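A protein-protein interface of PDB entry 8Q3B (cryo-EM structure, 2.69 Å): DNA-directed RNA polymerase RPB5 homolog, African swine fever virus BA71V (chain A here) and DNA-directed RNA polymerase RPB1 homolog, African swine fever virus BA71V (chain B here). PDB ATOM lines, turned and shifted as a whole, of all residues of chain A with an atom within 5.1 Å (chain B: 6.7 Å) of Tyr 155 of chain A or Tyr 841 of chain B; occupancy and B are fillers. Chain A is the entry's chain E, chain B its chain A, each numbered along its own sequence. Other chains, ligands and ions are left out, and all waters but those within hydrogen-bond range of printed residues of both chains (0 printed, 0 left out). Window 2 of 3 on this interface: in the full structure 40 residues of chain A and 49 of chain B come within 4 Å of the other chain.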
ATOM      1  N   PHE A 150      10.241   9.103  -9.675  1.00  0.00           N
ATOM      2  CA  PHE A 150      10.350   8.773 -11.091  1.00  0.00           C
ATOM      3  C   PHE A 150      11.341   7.637 -11.315  1.00  0.00           C
ATOM      4  O   PHE A 150      11.065   6.701 -12.076  1.00  0.00           O
ATOM      5  CB  PHE A 150      10.763  10.021 -11.873  1.00  0.00           C
ATOM      6  CG  PHE A 150      11.233   9.741 -13.270  1.00  0.00           C
ATOM      7  CD1 PHE A 150      10.325   9.552 -14.296  1.00  0.00           C
ATOM      8  CD2 PHE A 150      12.584   9.684 -13.561  1.00  0.00           C
ATOM      9  CE1 PHE A 150      10.756   9.303 -15.582  1.00  0.00           C
ATOM     10  CE2 PHE A 150      13.019   9.434 -14.845  1.00  0.00           C
ATOM     11  CZ  PHE A 150      12.105   9.243 -15.857  1.00  0.00           C
ATOM     12  N   LEU A 151      12.497   7.695 -10.651  1.00  0.00           N
ATOM     13  CA  LEU A 151      13.489   6.636 -10.796  1.00  0.00           C
ATOM     14  C   LEU A 151      12.954   5.306 -10.284  1.00  0.00           C
ATOM     15  O   LEU A 151      13.156   4.262 -10.916  1.00  0.00           O
ATOM     16  CB  LEU A 151      14.771   7.019 -10.058  1.00  0.00           C
ATOM     17  CG  LEU A 151      15.538   8.212 -10.630  1.00  0.00           C
ATOM     18  CD1 LEU A 151      16.630   8.647  -9.671  1.00  0.00           C
ATOM     19  CD2 LEU A 151      16.125   7.872 -11.988  1.00  0.00           C
ATOM     20  N   GLY A 152      12.271   5.319  -9.139  1.00  0.00           N
ATOM     21  CA  GLY A 152      11.713   4.087  -8.611  1.00  0.00           C
ATOM     22  C   GLY A 152      10.673   3.485  -9.534  1.00  0.00           C
ATOM     23  O   GLY A 152      10.635   2.269  -9.732  1.00  0.00           O
ATOM     24  N   ARG A 153       9.812   4.326 -10.110  1.00  0.00           N
ATOM     25  CA  ARG A 153       8.833   3.822 -11.066  1.00  0.00           C
ATOM     26  C   ARG A 153       9.518   3.243 -12.296  1.00  0.00           C
ATOM     27  O   ARG A 153       9.109   2.195 -12.808  1.00  0.00           O
ATOM     28  CB  ARG A 153       7.867   4.933 -11.471  1.00  0.00           C
ATOM     29  CG  ARG A 153       6.633   4.428 -12.198  1.00  0.00           C
ATOM     30  CD  ARG A 153       6.672   4.780 -13.674  1.00  0.00           C
ATOM     31  NE  ARG A 153       5.615   4.108 -14.420  1.00  0.00           N
ATOM     32  CZ  ARG A 153       5.673   3.819 -15.713  1.00  0.00           C
ATOM     33  NH1 ARG A 153       6.725   4.138 -16.448  1.00  0.00           N
ATOM     34  NH2 ARG A 153       4.649   3.191 -16.282  1.00  0.00           N
ATOM     35  N   GLU A 154      10.566   3.909 -12.782  1.00  0.00           N
ATOM     36  CA  GLU A 154      11.247   3.475 -13.995  1.00  0.00           C
ATOM     37  C   GLU A 154      12.322   2.427 -13.741  1.00  0.00           C
ATOM     38  O   GLU A 154      12.902   1.918 -14.706  1.00  0.00           O
ATOM     39  CB  GLU A 154      11.876   4.681 -14.696  1.00  0.00           C
ATOM     40  CG  GLU A 154      10.877   5.747 -15.112  1.00  0.00           C
ATOM     41  CD  GLU A 154      10.263   5.473 -16.469  1.00  0.00           C
ATOM     42  OE1 GLU A 154      11.002   5.063 -17.387  1.00  0.00           O
ATOM     43  OE2 GLU A 154       9.039   5.669 -16.620  1.00  0.00           O
ATOM     44  N   TYR A 155      12.604   2.088 -12.483  1.00  0.00           N
ATOM     45  CA  TYR A 155      13.666   1.138 -12.151  1.00  0.00           C
ATOM     46  C   TYR A 155      14.998   1.598 -12.739  1.00  0.00           C
ATOM     47  O   TYR A 155      15.666   0.869 -13.474  1.00  0.00           O
ATOM     48  CB  TYR A 155      13.312  -0.272 -12.632  1.00  0.00           C
ATOM     49  CG  TYR A 155      12.495  -1.077 -11.649  1.00  0.00           C
ATOM     50  CD1 TYR A 155      13.043  -1.508 -10.451  1.00  0.00           C
ATOM     51  CD2 TYR A 155      11.178  -1.412 -11.925  1.00  0.00           C
ATOM     52  CE1 TYR A 155      12.302  -2.246  -9.552  1.00  0.00           C
ATOM     53  CE2 TYR A 155      10.429  -2.149 -11.032  1.00  0.00           C
ATOM     54  CZ  TYR A 155      10.994  -2.564  -9.848  1.00  0.00           C
ATOM     55  OH  TYR A 155      10.251  -3.299  -8.955  1.00  0.00           O
ATOM     56  N   LEU A 156      15.383   2.828 -12.408  1.00  0.00           N
ATOM     57  CA  LEU A 156      16.581   3.445 -12.954  1.00  0.00           C
ATOM     58  C   LEU A 156      17.453   3.977 -11.827  1.00  0.00           C
ATOM     59  O   LEU A 156      16.979   4.274 -10.729  1.00  0.00           O
ATOM     60  CB  LEU A 156      16.235   4.595 -13.912  1.00  0.00           C
ATOM     61  CG  LEU A 156      15.811   4.224 -15.333  1.00  0.00           C
ATOM     62  CD1 LEU A 156      15.290   5.455 -16.051  1.00  0.00           C
ATOM     63  CD2 LEU A 156      16.960   3.603 -16.107  1.00  0.00           C
ATOM     64  N   GLN A 157      18.739   4.084 -12.118  1.00  0.00           N
ATOM     65  CA  GLN A 157      19.699   4.756 -11.264  1.00  0.00           C
ATOM     66  C   GLN A 157      19.978   6.150 -11.801  1.00  0.00           C
ATOM     67  O   GLN A 157      19.804   6.413 -12.994  1.00  0.00           O
ATOM     68  CB  GLN A 157      21.006   3.959 -11.193  1.00  0.00           C
ATOM     69  CG  GLN A 157      20.837   2.513 -10.756  1.00  0.00           C
ATOM     70  CD  GLN A 157      20.334   2.382  -9.330  1.00  0.00           C
ATOM     71  OE1 GLN A 157      19.400   1.631  -9.058  1.00  0.00           O
ATOM     72  NE2 GLN A 157      20.960   3.109  -8.412  1.00  0.00           N
ATOM     73  N   VAL B 838      15.280  -0.802 -28.078  1.00  0.00           N
ATOM     74  CA  VAL B 838      14.086  -0.485 -27.305  1.00  0.00           C
ATOM     75  C   VAL B 838      13.919  -1.514 -26.195  1.00  0.00           C
ATOM     76  O   VAL B 838      14.057  -2.722 -26.424  1.00  0.00           O
ATOM     77  CB  VAL B 838      12.850  -0.442 -28.215  1.00  0.00           C
ATOM     78  CG1 VAL B 838      11.603  -0.121 -27.412  1.00  0.00           C
ATOM     79  CG2 VAL B 838      13.043   0.574 -29.324  1.00  0.00           C
ATOM     80  N   ASP B 839      13.618  -1.041 -24.990  1.00  0.00           N
ATOM     81  CA  ASP B 839      13.462  -1.895 -23.821  1.00  0.00           C
ATOM     82  C   ASP B 839      11.990  -1.975 -23.422  1.00  0.00           C
ATOM     83  O   ASP B 839      11.105  -1.436 -24.091  1.00  0.00           O
ATOM     84  CB  ASP B 839      14.327  -1.385 -22.666  1.00  0.00           C
ATOM     85  CG  ASP B 839      14.029   0.052 -22.305  1.00  0.00           C
ATOM     86  OD1 ASP B 839      13.297   0.717 -23.065  1.00  0.00           O
ATOM     87  OD2 ASP B 839      14.532   0.520 -21.262  1.00  0.00           O
ATOM     88  N   TYR B 840      11.736  -2.663 -22.308  1.00  0.00           N
ATOM     89  CA  TYR B 840      10.374  -2.971 -21.890  1.00  0.00           C
ATOM     90  C   TYR B 840       9.572  -1.739 -21.497  1.00  0.00           C
ATOM     91  O   TYR B 840       8.342  -1.827 -21.409  1.00  0.00           O
ATOM     92  CB  TYR B 840      10.407  -3.961 -20.728  1.00  0.00           C
ATOM     93  CG  TYR B 840      10.876  -5.337 -21.136  1.00  0.00           C
ATOM     94  CD1 TYR B 840      10.204  -6.056 -22.111  1.00  0.00           C
ATOM     95  CD2 TYR B 840      11.996  -5.910 -20.556  1.00  0.00           C
ATOM     96  CE1 TYR B 840      10.629  -7.309 -22.493  1.00  0.00           C
ATOM     97  CE2 TYR B 840      12.430  -7.163 -20.931  1.00  0.00           C
ATOM     98  CZ  TYR B 840      11.742  -7.859 -21.900  1.00  0.00           C
ATOM     99  OH  TYR B 840      12.167  -9.109 -22.279  1.00  0.00           O
ATOM    100  N   TYR B 841      10.222  -0.606 -21.253  1.00  0.00           N
ATOM    101  CA  TYR B 841       9.529   0.654 -21.033  1.00  0.00           C
ATOM    102  C   TYR B 841       9.352   1.445 -22.321  1.00  0.00           C
ATOM    103  O   TYR B 841       8.885   2.587 -22.276  1.00  0.00           O
ATOM    104  CB  TYR B 841      10.288   1.499 -20.007  1.00  0.00           C
ATOM    105  CG  TYR B 841      10.142   1.021 -18.583  1.00  0.00           C
ATOM    106  CD1 TYR B 841      10.828  -0.096 -18.132  1.00  0.00           C
ATOM    107  CD2 TYR B 841       9.324   1.692 -17.687  1.00  0.00           C
ATOM    108  CE1 TYR B 841      10.700  -0.534 -16.832  1.00  0.00           C
ATOM    109  CE2 TYR B 841       9.189   1.261 -16.385  1.00  0.00           C
ATOM    110  CZ  TYR B 841       9.880   0.149 -15.962  1.00  0.00           C
ATOM    111  OH  TYR B 841       9.747  -0.283 -14.664  1.00  0.00           O
ATOM    112  N   ARG B 842       9.710   0.859 -23.463  1.00  0.00           N
ATOM    113  CA  ARG B 842       9.696   1.529 -24.760  1.00  0.00           C
ATOM    114  C   ARG B 842      10.637   2.727 -24.796  1.00  0.00           C
ATOM    115  O   ARG B 842      10.513   3.595 -25.665  1.00  0.00           O
ATOM    116  CB  ARG B 842       8.276   1.943 -25.159  1.00  0.00           C
ATOM    117  CG  ARG B 842       7.614   0.942 -26.092  1.00  0.00           C
ATOM    118  CD  ARG B 842       6.224   1.373 -26.506  1.00  0.00           C
ATOM    119  NE  ARG B 842       5.192   0.664 -25.762  1.00  0.00           N
ATOM    120  CZ  ARG B 842       4.725  -0.535 -26.084  1.00  0.00           C
ATOM    121  NH1 ARG B 842       5.193  -1.205 -27.124  1.00  0.00           N
ATOM    122  NH2 ARG B 842       3.765  -1.077 -25.341  1.00  0.00           N
ATOM    123  N   ARG B 843      11.585   2.782 -23.867  1.00  0.00           N
ATOM    124  CA  ARG B 843      12.680   3.730 -23.946  1.00  0.00           C
ATOM    125  C   ARG B 843      13.763   3.177 -24.863  1.00  0.00           C
ATOM    126  O   ARG B 843      13.724   2.019 -25.284  1.00  0.00           O
ATOM    127  CB  ARG B 843      13.261   4.008 -22.560  1.00  0.00           C
ATOM    128  CG  ARG B 843      12.234   4.072 -21.445  1.00  0.00           C
ATOM    129  CD  ARG B 843      12.891   4.324 -20.102  1.00  0.00           C
ATOM    130  NE  ARG B 843      13.732   3.204 -19.692  1.00  0.00           N
ATOM    131  CZ  ARG B 843      13.645   2.567 -18.530  1.00  0.00           C
ATOM    132  NH1 ARG B 843      12.761   2.914 -17.609  1.00  0.00           N
ATOM    133  NH2 ARG B 843      14.470   1.554 -18.285  1.00  0.00           N
ATOM    134  N   VAL B 844      14.743   4.016 -25.180  1.00  0.00           N
ATOM    135  CA  VAL B 844      15.908   3.600 -25.950  1.00  0.00           C
ATOM    136  C   VAL B 844      17.134   3.804 -25.076  1.00  0.00           C
ATOM    137  O   VAL B 844      17.374   4.916 -24.593  1.00  0.00           O
ATOM    138  CB  VAL B 844      16.034   4.380 -27.270  1.00  0.00           C
ATOM    139  CG1 VAL B 844      17.230   3.886 -28.052  1.00  0.00           C
ATOM    140  CG2 VAL B 844      14.764   4.247 -28.091  1.00  0.00           C
ATOM    141  N   GLN B 853      13.957   8.812 -23.662  1.00  0.00           N
ATOM    142  CA  GLN B 853      12.919   8.427 -22.714  1.00  0.00           C
ATOM    143  C   GLN B 853      11.811   7.634 -23.396  1.00  0.00           C
ATOM    144  O   GLN B 853      11.193   6.769 -22.769  1.00  0.00           O
ATOM    145  CB  GLN B 853      12.339   9.670 -22.041  1.00  0.00           C
ATOM    146  CG  GLN B 853      11.411   9.375 -20.877  1.00  0.00           C
ATOM    147  CD  GLN B 853      12.128   8.719 -19.715  1.00  0.00           C
ATOM    148  OE1 GLN B 853      13.040   9.300 -19.127  1.00  0.00           O
ATOM    149  NE2 GLN B 853      11.723   7.501 -19.378  1.00  0.00           N
ATOM    150  N   LEU B 854      11.538   7.924 -24.665  1.00  0.00           N
ATOM    151  CA  LEU B 854      10.541   7.192 -25.432  1.00  0.00           C
ATOM    152  C   LEU B 854      10.926   7.264 -26.903  1.00  0.00           C
ATOM    153  O   LEU B 854      11.247   8.339 -27.411  1.00  0.00           O
ATOM    154  CB  LEU B 854       9.137   7.765 -25.207  1.00  0.00           C
ATOM    155  CG  LEU B 854       7.965   6.931 -25.725  1.00  0.00           C
ATOM    156  CD1 LEU B 854       7.757   5.702 -24.860  1.00  0.00           C
ATOM    157  CD2 LEU B 854       6.698   7.767 -25.772  1.00  0.00           C
ATOM    158  N   TYR B 855      10.891   6.119 -27.579  1.00  0.00           N
ATOM    159  CA  TYR B 855      11.366   6.056 -28.955  1.00  0.00           C
ATOM    160  C   TYR B 855      10.533   6.961 -29.850  1.00  0.00           C
ATOM    161  O   TYR B 855       9.303   6.863 -29.882  1.00  0.00           O
ATOM    162  CB  TYR B 855      11.312   4.624 -29.482  1.00  0.00           C
ATOM    163  CG  TYR B 855      11.620   4.534 -30.958  1.00  0.00           C
ATOM    164  CD1 TYR B 855      12.865   4.896 -31.449  1.00  0.00           C
ATOM    165  CD2 TYR B 855      10.661   4.107 -31.864  1.00  0.00           C
ATOM    166  CE1 TYR B 855      13.151   4.824 -32.797  1.00  0.00           C
ATOM    167  CE2 TYR B 855      10.937   4.031 -33.214  1.00  0.00           C
ATOM    168  CZ  TYR B 855      12.183   4.391 -33.675  1.00  0.00           C
ATOM    169  OH  TYR B 855      12.464   4.318 -35.019  1.00  0.00           O
ATOM    170  N   PHE B 975       0.268   2.816 -23.506  1.00  0.00           N
ATOM    171  CA  PHE B 975       1.642   2.420 -23.228  1.00  0.00           C
ATOM    172  C   PHE B 975       1.718   1.526 -21.998  1.00  0.00           C
ATOM    173  O   PHE B 975       2.444   0.526 -21.989  1.00  0.00           O
ATOM    174  CB  PHE B 975       2.501   3.669 -23.052  1.00  0.00           C
ATOM    175  CG  PHE B 975       2.376   4.640 -24.188  1.00  0.00           C
ATOM    176  CD1 PHE B 975       2.925   4.349 -25.422  1.00  0.00           C
ATOM    177  CD2 PHE B 975       1.683   5.827 -24.032  1.00  0.00           C
ATOM    178  CE1 PHE B 975       2.805   5.231 -26.472  1.00  0.00           C
ATOM    179  CE2 PHE B 975       1.558   6.713 -25.081  1.00  0.00           C
ATOM    180  CZ  PHE B 975       2.119   6.414 -26.302  1.00  0.00           C
ATOM    181  N   TYR B 990       5.532  12.066 -19.163  1.00  0.00           N
ATOM    182  CA  TYR B 990       5.994  11.929 -20.539  1.00  0.00           C
ATOM    183  C   TYR B 990       5.052  11.067 -21.369  1.00  0.00           C
ATOM    184  O   TYR B 990       4.912  11.297 -22.576  1.00  0.00           O
ATOM    185  CB  TYR B 990       7.419  11.368 -20.565  1.00  0.00           C
ATOM    186  CG  TYR B 990       7.572   9.945 -20.079  1.00  0.00           C
ATOM    187  CD1 TYR B 990       7.618   9.656 -18.722  1.00  0.00           C
ATOM    188  CD2 TYR B 990       7.700   8.895 -20.976  1.00  0.00           C
ATOM    189  CE1 TYR B 990       7.770   8.360 -18.275  1.00  0.00           C
ATOM    190  CE2 TYR B 990       7.852   7.596 -20.537  1.00  0.00           C
ATOM    191  CZ  TYR B 990       7.887   7.334 -19.186  1.00  0.00           C
ATOM    192  OH  TYR B 990       8.038   6.042 -18.743  1.00  0.00           O
ATOM    193  N   LEU B 991       4.382  10.092 -20.755  1.00  0.00           N
ATOM    194  CA  LEU B 991       3.402   9.308 -21.500  1.00  0.00           C
ATOM    195  C   LEU B 991       2.192  10.155 -21.877  1.00  0.00           C
ATOM    196  O   LEU B 991       1.654  10.026 -22.985  1.00  0.00           O
ATOM    197  CB  LEU B 991       2.984   8.084 -20.684  1.00  0.00           C
ATOM    198  CG  LEU B 991       4.057   7.002 -20.514  1.00  0.00           C
ATOM    199  CD1 LEU B 991       3.498   5.803 -19.775  1.00  0.00           C
ATOM    200  CD2 LEU B 991       4.632   6.566 -21.853  1.00  0.00           C
ATOM    201  N   TYR B1037       9.406  -4.512 -28.398  1.00  0.00           N
ATOM    202  CA  TYR B1037      10.231  -4.430 -27.201  1.00  0.00           C
ATOM    203  C   TYR B1037      11.672  -4.873 -27.421  1.00  0.00           C
ATOM    204  O   TYR B1037      12.460  -4.836 -26.474  1.00  0.00           O
ATOM    205  CB  TYR B1037       9.607  -5.275 -26.084  1.00  0.00           C
ATOM    206  CG  TYR B1037       8.499  -4.592 -25.307  1.00  0.00           C
ATOM    207  CD1 TYR B1037       8.493  -3.216 -25.117  1.00  0.00           C
ATOM    208  CD2 TYR B1037       7.453  -5.327 -24.773  1.00  0.00           C
ATOM    209  CE1 TYR B1037       7.487  -2.600 -24.412  1.00  0.00           C
ATOM    210  CE2 TYR B1037       6.440  -4.715 -24.068  1.00  0.00           C
ATOM    211  CZ  TYR B1037       6.462  -3.351 -23.893  1.00  0.00           C
ATOM    212  OH  TYR B1037       5.459  -2.729 -23.193  1.00  0.00           O
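Of the 14 printed residues of chain B, 4 touch a printed residue of chain A.
Hydrophobic or aromatic side chains of chain B within 4 Å of the printed part of chain A: Tyr 841 and Tyr 990.
Printed residues of chain A that touch a printed residue of chain B: Phe 150, Arg 153, Glu 154, Tyr 155 and Leu 156.
Hydrophobic or aromatic side chains of chain A within 4 Å of the printed part of chain B: Phe 150, Tyr 155 and Leu 156.
Among the printed residues, 9 pairs touch across the chains.
Among the printed residues, Asp or Glu carboxylates within 4 Å of a Lys or Arg side-chain nitrogen of the other chain: Glu 154 of chain A with Arg 843 of chain B (2.8 Å).
Among the printed residues, merely in contact across the chains: Phe 150 of chain A with Gln 853 of chain B (3.4 Å), Glu 154 of chain A with Tyr 841 of chain B (3.7 Å), Tyr 155 of chain A with Tyr 841 of chain B (3.3 Å) and Leu 156 of chain A with Arg 843 of chain B (3.9 Å).
The backbone carbonyl oxygen (O) of Leu 151 of chain A sits at hydrogen-bond distance from the backbone NH (N) of Leu 156 of chain A (3.0 Å).
The side-chain carboxylate (OE2) of Glu 154 of chain A is in salt-bridge range of the guanidinium group (NH1) of Arg 153 of chain A (2.8 Å).
NH2 of Arg 843 of chain B lies within salt-bridge range of OD2 of Asp 839 of chain B (3.2 Å).
NH1 of Arg 153 of chain A is in hydrogen-bond range of OH of Tyr 990 of chain B (3.3 Å).
O of Arg 153 of chain A is in hydrogen-bond range of OH of Tyr 841 of chain B (3.2 Å).
The guanidinium group of Arg 843 of chain B lies within salt-bridge range of the side-chain carboxylate of Glu 154 of chain A (2.8 Å).
The side-chain amide nitrogen of Gln 853 of chain B sits at hydrogen-bond distance from the side-chain carboxylate of Glu 154 of chain A (3.2 Å).
OE1 of Glu 154 of chain A lies close to OH of Tyr 990 of chain B.
Of the printed residues of chain B, Arg 153 of chain A touches Tyr 841 (3.2 Å) and Tyr 990 (3.3 Å).
Of the printed residues of chain B, Tyr 155 of chain A touches Tyr 841 (3.3 Å).
Of chain A, only Arg 153, Glu 154 and Tyr 155 come within 4 Å of Tyr 841 of chain B.
Of the printed residues of chain A, Arg 843 of chain B touches Glu 154 (2.8 Å) and Leu 156 (3.9 Å).
Printed residues of chain A within 4 Å of Gln 853 of chain B: Phe 150 (3.4 Å) and Glu 154 (3.2 Å).
Leu 854 of chain B touches none of the printed residues of chain A.
The nearest printed residue of chain A that does not touch Tyr 841 of chain B is Gly 152 of chain A (5.6 Å).
The nearest printed residue of chain B that does not touch Arg 153 of chain A is Leu 991 of chain B (4.5 Å).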
